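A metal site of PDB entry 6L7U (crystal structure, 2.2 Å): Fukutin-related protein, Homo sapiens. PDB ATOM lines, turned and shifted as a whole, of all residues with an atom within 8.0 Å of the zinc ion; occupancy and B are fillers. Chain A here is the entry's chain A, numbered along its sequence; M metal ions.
O of Cys 249 is in hydrogen-bond range of NH2 of Arg 280. SG of Cys 256 sits close to NE of Arg 235, 3.4 Å away. The side-chain amide nitrogen (ND2) of Asn 371 lies close to the side-chain sulfur (SG) of Cys 249 (3.4 Å).
Merely in contact with the zinc ion: Pro 275. The nearest printed residue that does not touch the zinc ion is Gly 248 (4.8 Å).
The zinc ion is bound by the side-chain sulfur (SG) of Cys 277 (2.3 Å), the side-chain sulfur (SG) of Cys 278 (2.4 Å), the side-chain sulfur (SG) of Cys 249 (2.5 Å) and the side-chain sulfur (SG) of Cys 256 (2.5 Å).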
ATOM      1  N   ARG A 235      19.311 -32.154  10.127  1.00  0.00           N
ATOM      2  CA  ARG A 235      20.676 -32.067   9.617  1.00  0.00           C
ATOM      3  C   ARG A 235      21.260 -33.418   9.232  1.00  0.00           C
ATOM      4  O   ARG A 235      22.198 -33.462   8.433  1.00  0.00           O
ATOM      5  CB  ARG A 235      21.595 -31.430  10.664  1.00  0.00           C
ATOM      6  CG  ARG A 235      21.272 -29.990  10.967  1.00  0.00           C
ATOM      7  CD  ARG A 235      21.916 -29.059   9.979  1.00  0.00           C
ATOM      8  NE  ARG A 235      21.926 -27.703  10.493  1.00  0.00           N
ATOM      9  CZ  ARG A 235      20.907 -26.864  10.384  1.00  0.00           C
ATOM     10  NH1 ARG A 235      19.791 -27.247   9.769  1.00  0.00           N
ATOM     11  NH2 ARG A 235      21.001 -25.643  10.898  1.00  0.00           N
ATOM     12  N   TRP A 246      23.881 -36.190   5.178  1.00  0.00           N
ATOM     13  CA  TRP A 246      24.095 -34.931   5.859  1.00  0.00           C
ATOM     14  C   TRP A 246      23.449 -33.769   5.115  1.00  0.00           C
ATOM     15  O   TRP A 246      23.431 -33.743   3.881  1.00  0.00           O
ATOM     16  CB  TRP A 246      25.586 -34.636   6.040  1.00  0.00           C
ATOM     17  CG  TRP A 246      26.300 -35.651   6.873  1.00  0.00           C
ATOM     18  CD1 TRP A 246      27.009 -36.720   6.422  1.00  0.00           C
ATOM     19  CD2 TRP A 246      26.370 -35.684   8.302  1.00  0.00           C
ATOM     20  NE1 TRP A 246      27.529 -37.419   7.485  1.00  0.00           N
ATOM     21  CE2 TRP A 246      27.149 -36.810   8.656  1.00  0.00           C
ATOM     22  CE3 TRP A 246      25.859 -34.866   9.323  1.00  0.00           C
ATOM     23  CZ2 TRP A 246      27.429 -37.142   9.978  1.00  0.00           C
ATOM     24  CZ3 TRP A 246      26.133 -35.205  10.641  1.00  0.00           C
ATOM     25  CH2 TRP A 246      26.917 -36.327  10.953  1.00  0.00           C
ATOM     26  N   PHE A 247      22.933 -32.813   5.883  1.00  0.00           N
ATOM     27  CA  PHE A 247      22.310 -31.617   5.324  1.00  0.00           C
ATOM     28  C   PHE A 247      22.693 -30.367   6.111  1.00  0.00           C
ATOM     29  O   PHE A 247      21.910 -29.420   6.203  1.00  0.00           O
ATOM     30  CB  PHE A 247      20.784 -31.779   5.281  1.00  0.00           C
ATOM     31  CG  PHE A 247      20.338 -32.953   4.473  1.00  0.00           C
ATOM     32  CD1 PHE A 247      20.131 -32.831   3.101  1.00  0.00           C
ATOM     33  CD2 PHE A 247      20.154 -34.197   5.061  1.00  0.00           C
ATOM     34  CE1 PHE A 247      19.731 -33.922   2.351  1.00  0.00           C
ATOM     35  CE2 PHE A 247      19.767 -35.286   4.317  1.00  0.00           C
ATOM     36  CZ  PHE A 247      19.548 -35.145   2.953  1.00  0.00           C
ATOM     37  N   GLY A 248      23.910 -30.347   6.667  1.00  0.00           N
ATOM     38  CA  GLY A 248      24.356 -29.196   7.416  1.00  0.00           C
ATOM     39  C   GLY A 248      25.625 -28.565   6.879  1.00  0.00           C
ATOM     40  O   GLY A 248      25.761 -28.343   5.670  1.00  0.00           O
ATOM     41  N   CYS A 249      26.563 -28.261   7.775  1.00  0.00           N
ATOM     42  CA  CYS A 249      27.814 -27.619   7.400  1.00  0.00           C
ATOM     43  C   CYS A 249      28.877 -28.668   7.062  1.00  0.00           C
ATOM     44  O   CYS A 249      28.718 -29.857   7.331  1.00  0.00           O
ATOM     45  CB  CYS A 249      28.293 -26.708   8.525  1.00  0.00           C
ATOM     46  SG  CYS A 249      28.955 -27.566   9.964  1.00  0.00           S
ATOM     47  N   ASN A 250      29.969 -28.212   6.467  1.00  0.00           N
ATOM     48  CA  ASN A 250      31.086 -29.081   6.102  1.00  0.00           C
ATOM     49  C   ASN A 250      32.346 -28.249   5.973  1.00  0.00           C
ATOM     50  O   ASN A 250      32.358 -27.043   6.275  1.00  0.00           O
ATOM     51  CB  ASN A 250      30.782 -29.869   4.823  1.00  0.00           C
ATOM     52  CG  ASN A 250      30.486 -28.973   3.630  1.00  0.00           C
ATOM     53  OD1 ASN A 250      31.361 -28.255   3.144  1.00  0.00           O
ATOM     54  ND2 ASN A 250      29.253 -29.030   3.139  1.00  0.00           N
ATOM     55  N   THR A 253      31.897 -24.938   3.931  1.00  0.00           N
ATOM     56  CA  THR A 253      30.850 -23.975   4.276  1.00  0.00           C
ATOM     57  C   THR A 253      31.174 -23.288   5.585  1.00  0.00           C
ATOM     58  O   THR A 253      32.136 -23.611   6.280  1.00  0.00           O
ATOM     59  CB  THR A 253      29.479 -24.656   4.360  1.00  0.00           C
ATOM     60  OG1 THR A 253      29.383 -25.391   5.594  1.00  0.00           O
ATOM     61  CG2 THR A 253      29.276 -25.624   3.196  1.00  0.00           C
ATOM     62  N   THR A 254      30.335 -22.305   5.924  1.00  0.00           N
ATOM     63  CA  THR A 254      30.348 -21.749   7.262  1.00  0.00           C
ATOM     64  C   THR A 254      29.757 -22.761   8.242  1.00  0.00           C
ATOM     65  O   THR A 254      28.979 -23.643   7.862  1.00  0.00           O
ATOM     66  CB  THR A 254      29.578 -20.433   7.312  1.00  0.00           C
ATOM     67  OG1 THR A 254      29.736 -19.823   8.594  1.00  0.00           O
ATOM     68  CG2 THR A 254      28.087 -20.670   7.049  1.00  0.00           C
ATOM     69  N   ARG A 255      30.145 -22.635   9.503  1.00  0.00           N
ATOM     70  CA  ARG A 255      29.491 -23.448  10.514  1.00  0.00           C
ATOM     71  C   ARG A 255      28.035 -23.009  10.659  1.00  0.00           C
ATOM     72  O   ARG A 255      27.658 -21.893  10.279  1.00  0.00           O
ATOM     73  CB  ARG A 255      30.228 -23.362  11.854  1.00  0.00           C
ATOM     74  CG  ARG A 255      29.903 -22.148  12.710  1.00  0.00           C
ATOM     75  CD  ARG A 255      30.877 -22.045  13.878  1.00  0.00           C
ATOM     76  NE  ARG A 255      30.729 -20.805  14.634  1.00  0.00           N
ATOM     77  CZ  ARG A 255      31.509 -20.455  15.650  1.00  0.00           C
ATOM     78  NH1 ARG A 255      32.493 -21.253  16.041  1.00  0.00           N
ATOM     79  NH2 ARG A 255      31.309 -19.300  16.278  1.00  0.00           N
ATOM     80  N   CYS A 256      27.209 -23.912  11.188  1.00  0.00           N
ATOM     81  CA  CYS A 256      25.764 -23.705  11.158  1.00  0.00           C
ATOM     82  C   CYS A 256      25.351 -22.453  11.919  1.00  0.00           C
ATOM     83  O   CYS A 256      24.549 -21.657  11.416  1.00  0.00           O
ATOM     84  CB  CYS A 256      25.046 -24.929  11.718  1.00  0.00           C
ATOM     85  SG  CYS A 256      25.067 -26.345  10.602  1.00  0.00           S
ATOM     86  N   PHE A 257      25.880 -22.265  13.113  1.00  0.00           N
ATOM     87  CA  PHE A 257      25.373 -21.204  13.980  1.00  0.00           C
ATOM     88  C   PHE A 257      26.138 -19.888  13.851  1.00  0.00           C
ATOM     89  O   PHE A 257      25.813 -18.937  14.557  1.00  0.00           O
ATOM     90  CB  PHE A 257      25.377 -21.660  15.450  1.00  0.00           C
ATOM     91  CG  PHE A 257      26.675 -22.252  15.926  1.00  0.00           C
ATOM     92  CD1 PHE A 257      26.946 -23.600  15.735  1.00  0.00           C
ATOM     93  CD2 PHE A 257      27.610 -21.476  16.584  1.00  0.00           C
ATOM     94  CE1 PHE A 257      28.124 -24.150  16.179  1.00  0.00           C
ATOM     95  CE2 PHE A 257      28.794 -22.019  17.032  1.00  0.00           C
ATOM     96  CZ  PHE A 257      29.057 -23.366  16.826  1.00  0.00           C
ATOM     97  N   THR A 274      23.575 -28.871  19.868  1.00  0.00           N
ATOM     98  CA  THR A 274      24.512 -28.604  18.797  1.00  0.00           C
ATOM     99  C   THR A 274      24.170 -29.457  17.569  1.00  0.00           C
ATOM    100  O   THR A 274      23.869 -30.647  17.711  1.00  0.00           O
ATOM    101  CB  THR A 274      25.945 -28.890  19.249  1.00  0.00           C
ATOM    102  OG1 THR A 274      26.185 -28.225  20.490  1.00  0.00           O
ATOM    103  CG2 THR A 274      26.957 -28.398  18.214  1.00  0.00           C
ATOM    104  N   PRO A 275      24.157 -28.864  16.373  1.00  0.00           N
ATOM    105  CA  PRO A 275      23.909 -29.646  15.156  1.00  0.00           C
ATOM    106  C   PRO A 275      24.904 -30.783  15.008  1.00  0.00           C
ATOM    107  O   PRO A 275      26.092 -30.623  15.344  1.00  0.00           O
ATOM    108  CB  PRO A 275      24.065 -28.602  14.030  1.00  0.00           C
ATOM    109  CG  PRO A 275      23.715 -27.307  14.693  1.00  0.00           C
ATOM    110  CD  PRO A 275      24.198 -27.423  16.113  1.00  0.00           C
ATOM    111  N   PRO A 276      24.465 -31.937  14.511  1.00  0.00           N
ATOM    112  CA  PRO A 276      25.368 -33.096  14.437  1.00  0.00           C
ATOM    113  C   PRO A 276      26.488 -32.926  13.433  1.00  0.00           C
ATOM    114  O   PRO A 276      27.543 -33.551  13.579  1.00  0.00           O
ATOM    115  CB  PRO A 276      24.424 -34.250  14.059  1.00  0.00           C
ATOM    116  CG  PRO A 276      23.279 -33.586  13.354  1.00  0.00           C
ATOM    117  CD  PRO A 276      23.111 -32.239  14.015  1.00  0.00           C
ATOM    118  N   CYS A 277      26.294 -32.102  12.404  1.00  0.00           N
ATOM    119  CA  CYS A 277      27.382 -31.766  11.498  1.00  0.00           C
ATOM    120  C   CYS A 277      28.462 -30.953  12.211  1.00  0.00           C
ATOM    121  O   CYS A 277      29.654 -31.119  11.939  1.00  0.00           O
ATOM    122  CB  CYS A 277      26.851 -30.998  10.292  1.00  0.00           C
ATOM    123  SG  CYS A 277      25.771 -29.624  10.793  1.00  0.00           S
ATOM    124  N   CYS A 278      28.045 -30.066  13.120  1.00  0.00           N
ATOM    125  CA  CYS A 278      29.011 -29.282  13.874  1.00  0.00           C
ATOM    126  C   CYS A 278      29.785 -30.163  14.858  1.00  0.00           C
ATOM    127  O   CYS A 278      30.994 -29.985  15.027  1.00  0.00           O
ATOM    128  CB  CYS A 278      28.307 -28.147  14.607  1.00  0.00           C
ATOM    129  SG  CYS A 278      27.544 -26.885  13.537  1.00  0.00           S
ATOM    130  N   LEU A 279      29.098 -31.102  15.508  1.00  0.00           N
ATOM    131  CA  LEU A 279      29.799 -32.037  16.391  1.00  0.00           C
ATOM    132  C   LEU A 279      30.743 -32.940  15.619  1.00  0.00           C
ATOM    133  O   LEU A 279      31.865 -33.218  16.074  1.00  0.00           O
ATOM    134  CB  LEU A 279      28.775 -32.870  17.180  1.00  0.00           C
ATOM    135  CG  LEU A 279      27.969 -32.087  18.207  1.00  0.00           C
ATOM    136  CD1 LEU A 279      26.893 -32.967  18.850  1.00  0.00           C
ATOM    137  CD2 LEU A 279      28.887 -31.493  19.259  1.00  0.00           C
ATOM    138  N   ARG A 280      30.325 -33.397  14.431  1.00  0.00           N
ATOM    139  CA  ARG A 280      31.180 -34.246  13.611  1.00  0.00           C
ATOM    140  C   ARG A 280      32.471 -33.530  13.244  1.00  0.00           C
ATOM    141  O   ARG A 280      33.567 -34.098  13.351  1.00  0.00           O
ATOM    142  CB  ARG A 280      30.451 -34.696  12.347  1.00  0.00           C
ATOM    143  CG  ARG A 280      31.337 -35.394  11.328  1.00  0.00           C
ATOM    144  CD  ARG A 280      30.709 -35.459   9.944  1.00  0.00           C
ATOM    145  NE  ARG A 280      30.463 -34.134   9.367  1.00  0.00           N
ATOM    146  CZ  ARG A 280      29.966 -33.925   8.155  1.00  0.00           C
ATOM    147  NH1 ARG A 280      29.649 -34.955   7.376  1.00  0.00           N
ATOM    148  NH2 ARG A 280      29.768 -32.689   7.725  1.00  0.00           N
ATOM    149  N   ALA A 281      32.370 -32.270  12.809  1.00  0.00           N
ATOM    150  CA  ALA A 281      33.562 -31.490  12.491  1.00  0.00           C
ATOM    151  C   ALA A 281      34.429 -31.282  13.722  1.00  0.00           C
ATOM    152  O   ALA A 281      35.668 -31.260  13.624  1.00  0.00           O
ATOM    153  CB  ALA A 281      33.169 -30.153  11.876  1.00  0.00           C
ATOM    154  N   ASN A 371      34.963 -22.731   7.923  1.00  0.00           N
ATOM    155  CA  ASN A 371      34.192 -23.327   9.008  1.00  0.00           C
ATOM    156  C   ASN A 371      34.958 -23.164  10.317  1.00  0.00           C
ATOM    157  O   ASN A 371      35.935 -23.876  10.559  1.00  0.00           O
ATOM    158  CB  ASN A 371      33.904 -24.800   8.710  1.00  0.00           C
ATOM    159  CG  ASN A 371      32.878 -25.399   9.656  1.00  0.00           C
ATOM    160  OD1 ASN A 371      32.905 -25.157  10.865  1.00  0.00           O
ATOM    161  ND2 ASN A 371      31.960 -26.191   9.105  1.00  0.00           N
ATOM    162  N   LEU A 373      34.521 -23.879  13.458  1.00  0.00           N
ATOM    163  CA  LEU A 373      34.517 -24.775  14.603  1.00  0.00           C
ATOM    164  C   LEU A 373      35.960 -25.115  14.961  1.00  0.00           C
ATOM    165  O   LEU A 373      36.774 -25.397  14.066  1.00  0.00           O
ATOM    166  CB  LEU A 373      33.718 -26.037  14.293  1.00  0.00           C
ATOM    167  CG  LEU A 373      32.235 -25.795  14.024  1.00  0.00           C
ATOM    168  CD1 LEU A 373      31.640 -26.941  13.224  1.00  0.00           C
ATOM    169  CD2 LEU A 373      31.475 -25.590  15.319  1.00  0.00           C
HETATM  170 ZN    ZN M   1      26.951 -27.752  11.413  1.00  0.00          ZN
